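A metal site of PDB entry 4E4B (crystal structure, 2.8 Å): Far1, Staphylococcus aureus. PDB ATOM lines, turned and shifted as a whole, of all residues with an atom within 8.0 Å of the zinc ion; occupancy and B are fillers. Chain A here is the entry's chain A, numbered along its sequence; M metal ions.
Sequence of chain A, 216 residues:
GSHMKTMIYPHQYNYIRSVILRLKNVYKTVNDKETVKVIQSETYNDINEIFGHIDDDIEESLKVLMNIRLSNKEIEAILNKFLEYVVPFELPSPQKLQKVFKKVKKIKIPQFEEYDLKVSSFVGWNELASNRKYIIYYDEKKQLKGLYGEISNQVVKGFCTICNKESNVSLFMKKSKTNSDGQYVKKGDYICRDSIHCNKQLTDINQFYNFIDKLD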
ATOM      1  N   PHE A 122     -13.973  20.797  11.825  1.00  0.00           N
ATOM      2  CA  PHE A 122     -12.764  20.812  11.006  1.00  0.00           C
ATOM      3  C   PHE A 122     -12.536  22.234  10.525  1.00  0.00           C
ATOM      4  O   PHE A 122     -13.415  23.091  10.676  1.00  0.00           O
ATOM      5  CB  PHE A 122     -12.895  19.868   9.806  1.00  0.00           C
ATOM      6  CG  PHE A 122     -13.956  20.282   8.825  1.00  0.00           C
ATOM      7  CD1 PHE A 122     -13.614  20.962   7.663  1.00  0.00           C
ATOM      8  CD2 PHE A 122     -15.292  20.004   9.070  1.00  0.00           C
ATOM      9  CE1 PHE A 122     -14.585  21.352   6.753  1.00  0.00           C
ATOM     10  CE2 PHE A 122     -16.284  20.398   8.157  1.00  0.00           C
ATOM     11  CZ  PHE A 122     -15.921  21.074   6.998  1.00  0.00           C
ATOM     12  N   GLY A 158     -26.920  22.458  -4.261  1.00  0.00           N
ATOM     13  CA  GLY A 158     -26.844  21.013  -4.117  1.00  0.00           C
ATOM     14  C   GLY A 158     -26.422  20.650  -2.715  1.00  0.00           C
ATOM     15  O   GLY A 158     -25.876  21.487  -1.982  1.00  0.00           O
ATOM     16  N   PHE A 159     -26.676  19.400  -2.340  1.00  0.00           N
ATOM     17  CA  PHE A 159     -26.377  18.949  -0.987  1.00  0.00           C
ATOM     18  C   PHE A 159     -24.882  18.723  -0.814  1.00  0.00           C
ATOM     19  O   PHE A 159     -24.222  18.162  -1.692  1.00  0.00           O
ATOM     20  CB  PHE A 159     -27.187  17.689  -0.660  1.00  0.00           C
ATOM     21  CG  PHE A 159     -28.675  17.907  -0.678  1.00  0.00           C
ATOM     22  CD1 PHE A 159     -29.385  18.043   0.517  1.00  0.00           C
ATOM     23  CD2 PHE A 159     -29.372  17.992  -1.885  1.00  0.00           C
ATOM     24  CE1 PHE A 159     -30.759  18.258   0.498  1.00  0.00           C
ATOM     25  CE2 PHE A 159     -30.747  18.206  -1.903  1.00  0.00           C
ATOM     26  CZ  PHE A 159     -31.444  18.336  -0.705  1.00  0.00           C
ATOM     27  N   CYS A 160     -24.358  19.196   0.309  1.00  0.00           N
ATOM     28  CA  CYS A 160     -22.964  18.981   0.645  1.00  0.00           C
ATOM     29  C   CYS A 160     -22.827  17.600   1.256  1.00  0.00           C
ATOM     30  O   CYS A 160     -23.551  17.265   2.180  1.00  0.00           O
ATOM     31  CB  CYS A 160     -22.508  20.041   1.636  1.00  0.00           C
ATOM     32  SG  CYS A 160     -21.035  19.585   2.579  1.00  0.00           S
ATOM     33  N   THR A 161     -21.891  16.807   0.757  1.00  0.00           N
ATOM     34  CA  THR A 161     -21.697  15.426   1.231  1.00  0.00           C
ATOM     35  C   THR A 161     -20.973  15.334   2.584  1.00  0.00           C
ATOM     36  O   THR A 161     -20.663  14.233   3.037  1.00  0.00           O
ATOM     37  CB  THR A 161     -21.009  14.527   0.181  1.00  0.00           C
ATOM     38  OG1 THR A 161     -19.684  15.011  -0.075  1.00  0.00           O
ATOM     39  N   ILE A 162     -20.694  16.481   3.211  1.00  0.00           N
ATOM     40  CA  ILE A 162     -20.173  16.504   4.588  1.00  0.00           C
ATOM     41  C   ILE A 162     -21.275  16.868   5.592  1.00  0.00           C
ATOM     42  O   ILE A 162     -21.643  16.050   6.430  1.00  0.00           O
ATOM     43  CB  ILE A 162     -18.992  17.492   4.750  1.00  0.00           C
ATOM     44  CG1 ILE A 162     -17.742  16.942   4.053  1.00  0.00           C
ATOM     45  CG2 ILE A 162     -18.716  17.763   6.223  1.00  0.00           C
ATOM     46  CD1 ILE A 162     -16.570  17.910   4.071  1.00  0.00           C
ATOM     47  N   CYS A 163     -21.809  18.086   5.487  1.00  0.00           N
ATOM     48  CA  CYS A 163     -22.843  18.537   6.417  1.00  0.00           C
ATOM     49  C   CYS A 163     -24.208  18.008   6.005  1.00  0.00           C
ATOM     50  O   CYS A 163     -25.184  18.166   6.746  1.00  0.00           O
ATOM     51  CB  CYS A 163     -22.871  20.059   6.472  1.00  0.00           C
ATOM     52  SG  CYS A 163     -23.444  20.804   4.931  1.00  0.00           S
ATOM     53  N   ASN A 164     -24.273  17.383   4.827  1.00  0.00           N
ATOM     54  CA  ASN A 164     -25.502  16.825   4.241  1.00  0.00           C
ATOM     55  C   ASN A 164     -26.682  17.777   4.123  1.00  0.00           C
ATOM     56  O   ASN A 164     -27.834  17.358   4.192  1.00  0.00           O
ATOM     57  CB  ASN A 164     -25.911  15.534   4.948  1.00  0.00           C
ATOM     58  CG  ASN A 164     -24.954  14.391   4.662  1.00  0.00           C
ATOM     59  OD1 ASN A 164     -24.153  14.013   5.522  1.00  0.00           O
ATOM     60  ND2 ASN A 164     -25.020  13.847   3.440  1.00  0.00           N
ATOM     61  N   LYS A 165     -26.378  19.052   3.927  1.00  0.00           N
ATOM     62  CA  LYS A 165     -27.410  20.067   3.761  1.00  0.00           C
ATOM     63  C   LYS A 165     -27.217  20.829   2.466  1.00  0.00           C
ATOM     64  O   LYS A 165     -26.081  21.105   2.054  1.00  0.00           O
ATOM     65  CB  LYS A 165     -27.451  21.000   4.964  1.00  0.00           C
ATOM     66  CG  LYS A 165     -28.213  20.435   6.155  1.00  0.00           C
ATOM     67  CD  LYS A 165     -27.824  21.103   7.469  1.00  0.00           C
ATOM     68  CE  LYS A 165     -28.486  22.459   7.677  1.00  0.00           C
ATOM     69  NZ  LYS A 165     -29.744  22.391   8.481  1.00  0.00           N
ATOM     70  N   GLU A 166     -28.329  21.159   1.810  1.00  0.00           N
ATOM     71  CA  GLU A 166     -28.301  21.883   0.552  1.00  0.00           C
ATOM     72  C   GLU A 166     -27.587  23.216   0.730  1.00  0.00           C
ATOM     73  O   GLU A 166     -27.924  24.009   1.611  1.00  0.00           O
ATOM     74  CB  GLU A 166     -29.704  22.107  -0.016  1.00  0.00           C
ATOM     75  CG  GLU A 166     -29.703  22.204  -1.536  1.00  0.00           C
ATOM     76  CD  GLU A 166     -30.905  22.947  -2.089  1.00  0.00           C
ATOM     77  OE1 GLU A 166     -31.646  23.572  -1.298  1.00  0.00           O
ATOM     78  OE2 GLU A 166     -31.091  22.920  -3.320  1.00  0.00           O
ATOM     79  N   SER A 167     -26.585  23.435  -0.114  1.00  0.00           N
ATOM     80  CA  SER A 167     -25.654  24.521   0.087  1.00  0.00           C
ATOM     81  C   SER A 167     -25.030  24.914  -1.260  1.00  0.00           C
ATOM     82  O   SER A 167     -25.390  24.370  -2.308  1.00  0.00           O
ATOM     83  CB  SER A 167     -24.581  24.063   1.087  1.00  0.00           C
ATOM     84  OG  SER A 167     -23.774  25.139   1.544  1.00  0.00           O
ATOM     85  N   ASN A 168     -24.125  25.879  -1.217  1.00  0.00           N
ATOM     86  CA  ASN A 168     -23.347  26.257  -2.383  1.00  0.00           C
ATOM     87  C   ASN A 168     -22.119  25.378  -2.433  1.00  0.00           C
ATOM     88  O   ASN A 168     -21.137  25.622  -1.724  1.00  0.00           O
ATOM     89  CB  ASN A 168     -22.962  27.733  -2.321  1.00  0.00           C
ATOM     90  CG  ASN A 168     -24.157  28.655  -2.167  1.00  0.00           C
ATOM     91  OD1 ASN A 168     -25.269  28.348  -2.610  1.00  0.00           O
ATOM     92  ND2 ASN A 168     -23.938  29.799  -1.511  1.00  0.00           N
ATOM     93  N   VAL A 169     -22.186  24.349  -3.278  1.00  0.00           N
ATOM     94  CA  VAL A 169     -21.163  23.306  -3.297  1.00  0.00           C
ATOM     95  C   VAL A 169     -20.232  23.393  -4.503  1.00  0.00           C
ATOM     96  O   VAL A 169     -20.608  23.903  -5.572  1.00  0.00           O
ATOM     97  CB  VAL A 169     -21.765  21.890  -3.193  1.00  0.00           C
ATOM     98  CG1 VAL A 169     -22.522  21.735  -1.891  1.00  0.00           C
ATOM     99  CG2 VAL A 169     -22.678  21.601  -4.379  1.00  0.00           C
ATOM    100  N   TYR A 190     -19.013  16.640  -3.981  1.00  0.00           N
ATOM    101  CA  TYR A 190     -19.436  17.998  -3.680  1.00  0.00           C
ATOM    102  C   TYR A 190     -19.445  18.256  -2.191  1.00  0.00           C
ATOM    103  O   TYR A 190     -19.951  17.444  -1.410  1.00  0.00           O
ATOM    104  CB  TYR A 190     -20.812  18.272  -4.278  1.00  0.00           C
ATOM    105  CG  TYR A 190     -20.762  18.385  -5.789  1.00  0.00           C
ATOM    106  CD1 TYR A 190     -20.240  19.523  -6.402  1.00  0.00           C
ATOM    107  CD2 TYR A 190     -21.195  17.336  -6.588  1.00  0.00           C
ATOM    108  CE1 TYR A 190     -20.172  19.619  -7.785  1.00  0.00           C
ATOM    109  CE2 TYR A 190     -21.126  17.428  -7.980  1.00  0.00           C
ATOM    110  CZ  TYR A 190     -20.615  18.571  -8.574  1.00  0.00           C
ATOM    111  OH  TYR A 190     -20.555  18.659  -9.944  1.00  0.00           O
ATOM    112  N   ILE A 191     -18.848  19.381  -1.804  1.00  0.00           N
ATOM    113  CA  ILE A 191     -18.857  19.873  -0.424  1.00  0.00           C
ATOM    114  C   ILE A 191     -19.002  21.401  -0.413  1.00  0.00           C
ATOM    115  O   ILE A 191     -18.601  22.074  -1.372  1.00  0.00           O
ATOM    116  CB  ILE A 191     -17.581  19.484   0.356  1.00  0.00           C
ATOM    117  CG1 ILE A 191     -16.345  20.204  -0.202  1.00  0.00           C
ATOM    118  CG2 ILE A 191     -17.397  17.967   0.398  1.00  0.00           C
ATOM    119  CD1 ILE A 191     -15.121  20.119   0.686  1.00  0.00           C
ATOM    120  N   CYS A 192     -19.555  21.934   0.671  1.00  0.00           N
ATOM    121  CA  CYS A 192     -19.641  23.376   0.885  1.00  0.00           C
ATOM    122  C   CYS A 192     -18.344  24.081   0.512  1.00  0.00           C
ATOM    123  O   CYS A 192     -17.269  23.758   0.999  1.00  0.00           O
ATOM    124  CB  CYS A 192     -19.972  23.681   2.341  1.00  0.00           C
ATOM    125  SG  CYS A 192     -21.680  23.307   2.795  1.00  0.00           S
ATOM    126  N   ARG A 193     -18.467  25.041  -0.400  1.00  0.00           N
ATOM    127  CA  ARG A 193     -17.331  25.804  -0.853  1.00  0.00           C
ATOM    128  C   ARG A 193     -16.709  26.553   0.325  1.00  0.00           C
ATOM    129  O   ARG A 193     -15.489  26.563   0.487  1.00  0.00           O
ATOM    130  CB  ARG A 193     -17.750  26.768  -1.963  1.00  0.00           C
ATOM    131  CG  ARG A 193     -16.566  27.535  -2.512  1.00  0.00           C
ATOM    132  CD  ARG A 193     -16.798  28.132  -3.878  1.00  0.00           C
ATOM    133  NE  ARG A 193     -15.507  28.508  -4.461  1.00  0.00           N
ATOM    134  CZ  ARG A 193     -14.731  27.673  -5.140  1.00  0.00           C
ATOM    135  NH1 ARG A 193     -15.124  26.415  -5.337  1.00  0.00           N
ATOM    136  NH2 ARG A 193     -13.578  28.077  -5.626  1.00  0.00           N
ATOM    137  N   ASP A 194     -17.562  27.180   1.139  1.00  0.00           N
ATOM    138  CA  ASP A 194     -17.129  27.865   2.362  1.00  0.00           C
ATOM    139  C   ASP A 194     -17.268  26.915   3.555  1.00  0.00           C
ATOM    140  O   ASP A 194     -18.378  26.536   3.947  1.00  0.00           O
ATOM    141  CB  ASP A 194     -17.949  29.149   2.578  1.00  0.00           C
ATOM    142  CG  ASP A 194     -17.905  29.645   4.014  1.00  0.00           C
ATOM    143  OD1 ASP A 194     -16.865  30.198   4.447  1.00  0.00           O
ATOM    144  OD2 ASP A 194     -18.937  29.484   4.701  1.00  0.00           O
ATOM    145  N   SER A 195     -16.131  26.519   4.121  1.00  0.00           N
ATOM    146  CA  SER A 195     -16.129  25.479   5.156  1.00  0.00           C
ATOM    147  C   SER A 195     -16.659  25.909   6.501  1.00  0.00           C
ATOM    148  O   SER A 195     -17.096  25.068   7.278  1.00  0.00           O
ATOM    149  CB  SER A 195     -14.733  24.906   5.315  1.00  0.00           C
ATOM    150  OG  SER A 195     -14.454  24.071   4.219  1.00  0.00           O
ATOM    151  N   ILE A 196     -16.625  27.210   6.784  1.00  0.00           N
ATOM    152  CA  ILE A 196     -17.156  27.676   8.060  1.00  0.00           C
ATOM    153  C   ILE A 196     -18.676  27.487   8.080  1.00  0.00           C
ATOM    154  O   ILE A 196     -19.244  27.078   9.101  1.00  0.00           O
ATOM    155  CB  ILE A 196     -16.676  29.103   8.464  1.00  0.00           C
ATOM    156  CG1 ILE A 196     -17.295  30.196   7.590  1.00  0.00           C
ATOM    157  CG2 ILE A 196     -15.154  29.200   8.439  1.00  0.00           C
ATOM    158  CD1 ILE A 196     -18.347  31.022   8.284  1.00  0.00           C
ATOM    159  N   HIS A 197     -19.327  27.726   6.942  1.00  0.00           N
ATOM    160  CA  HIS A 197     -20.770  27.459   6.816  1.00  0.00           C
ATOM    161  C   HIS A 197     -21.082  26.004   6.991  1.00  0.00           C
ATOM    162  O   HIS A 197     -22.030  25.633   7.685  1.00  0.00           O
ATOM    163  CB  HIS A 197     -21.293  27.946   5.475  1.00  0.00           C
ATOM    164  CG  HIS A 197     -22.782  27.776   5.316  1.00  0.00           C
ATOM    165  ND1 HIS A 197     -23.670  28.595   5.896  1.00  0.00           N
ATOM    166  CD2 HIS A 197     -23.522  26.815   4.621  1.00  0.00           C
ATOM    167  CE1 HIS A 197     -24.918  28.189   5.592  1.00  0.00           C
ATOM    168  NE2 HIS A 197     -24.826  27.107   4.814  1.00  0.00           N
ATOM    169  N   CYS A 198     -20.273  25.166   6.337  1.00  0.00           N
ATOM    170  CA  CYS A 198     -20.360  23.711   6.452  1.00  0.00           C
ATOM    171  C   CYS A 198     -20.350  23.315   7.924  1.00  0.00           C
ATOM    172  O   CYS A 198     -21.253  22.609   8.392  1.00  0.00           O
ATOM    173  CB  CYS A 198     -19.140  23.120   5.758  1.00  0.00           C
ATOM    174  SG  CYS A 198     -19.272  21.397   5.265  1.00  0.00           S
ATOM    175  N   ASN A 199     -19.332  23.785   8.639  1.00  0.00           N
ATOM    176  CA  ASN A 199     -19.192  23.603  10.085  1.00  0.00           C
ATOM    177  C   ASN A 199     -20.408  24.068  10.875  1.00  0.00           C
ATOM    178  O   ASN A 199     -20.892  23.348  11.750  1.00  0.00           O
ATOM    179  CB  ASN A 199     -17.960  24.348  10.582  1.00  0.00           C
ATOM    180  CG  ASN A 199     -16.675  23.592  10.342  1.00  0.00           C
ATOM    181  OD1 ASN A 199     -16.613  22.373  10.522  1.00  0.00           O
ATOM    182  ND2 ASN A 199     -15.629  24.313   9.976  1.00  0.00           N
ATOM    183  N   LYS A 200     -20.901  25.263  10.565  1.00  0.00           N
ATOM    184  CA  LYS A 200     -22.085  25.829  11.207  1.00  0.00           C
ATOM    185  C   LYS A 200     -23.242  24.846  11.197  1.00  0.00           C
ATOM    186  O   LYS A 200     -24.068  24.837  12.106  1.00  0.00           O
ATOM    187  CB  LYS A 200     -22.513  27.128  10.533  1.00  0.00           C
ATOM    188  CG  LYS A 200     -21.712  28.348  10.939  1.00  0.00           C
ATOM    189  CD  LYS A 200     -22.167  29.581  10.181  1.00  0.00           C
ATOM    190  CE  LYS A 200     -21.734  30.863  10.871  1.00  0.00           C
ATOM    191  NZ  LYS A 200     -20.258  30.963  11.058  1.00  0.00           N
ATOM    192  N   GLN A 201     -23.303  24.015  10.160  1.00  0.00           N
ATOM    193  CA  GLN A 201     -24.385  23.048  10.040  1.00  0.00           C
ATOM    194  C   GLN A 201     -23.908  21.606  10.180  1.00  0.00           C
ATOM    195  O   GLN A 201     -24.682  20.679   9.990  1.00  0.00           O
ATOM    196  CB  GLN A 201     -25.160  23.266   8.749  1.00  0.00           C
ATOM    197  CG  GLN A 201     -24.313  23.481   7.504  1.00  0.00           C
ATOM    198  CD  GLN A 201     -25.109  24.098   6.393  1.00  0.00           C
ATOM    199  OE1 GLN A 201     -26.039  24.877   6.627  1.00  0.00           O
ATOM    200  NE2 GLN A 201     -24.755  23.766   5.145  1.00  0.00           N
ATOM    201  N   LEU A 202     -22.647  21.434  10.542  1.00  0.00           N
ATOM    202  CA  LEU A 202     -22.135  20.130  10.899  1.00  0.00           C
ATOM    203  C   LEU A 202     -22.613  19.697  12.296  1.00  0.00           C
ATOM    204  O   LEU A 202     -22.013  20.057  13.320  1.00  0.00           O
ATOM    205  CB  LEU A 202     -20.602  20.088  10.781  1.00  0.00           C
ATOM    206  CG  LEU A 202     -19.964  18.687  10.764  1.00  0.00           C
ATOM    207  CD1 LEU A 202     -20.599  17.799   9.709  1.00  0.00           C
ATOM    208  CD2 LEU A 202     -18.461  18.797  10.547  1.00  0.00           C
HETATM  209 ZN    ZN M   1     -21.335  21.438   4.214  1.00  0.00          ZN
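The side-chain sulfur of Cys 163 lies close to the side-chain amide nitrogen of Gln 201, at 3.2 Å. The backbone NH (N) of Cys 160 lies within hydrogen-bond range of the backbone carbonyl oxygen (O) of Lys 165. SG of Cys 192 lies close to OG of Ser 167. The backbone NH (N) of Lys 165 lies close to the side-chain sulfur (SG) of Cys 163, at 3.6 Å. The side-chain sulfur (SG) of Cys 160 sits close to the backbone NH (N) of Ile 162 (3.2 Å).
Within 4 Å of the zinc ion: Cys 160, Cys 163, Cys 192 and Cys 198. The nearest printed residue that does not touch the zinc ion is Gln 201 (4.2 Å).
The side-chain sulfur (SG) of Cys 198 is bound to the zinc ion (2.3 Å). SG of Cys 163 binds the zinc ion, 2.3 Å away. SG of Cys 192 binds the zinc ion. SG of Cys 160 is bound to the zinc ion, at 2.5 Å. The zinc ion has four donor atoms within binding distance.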
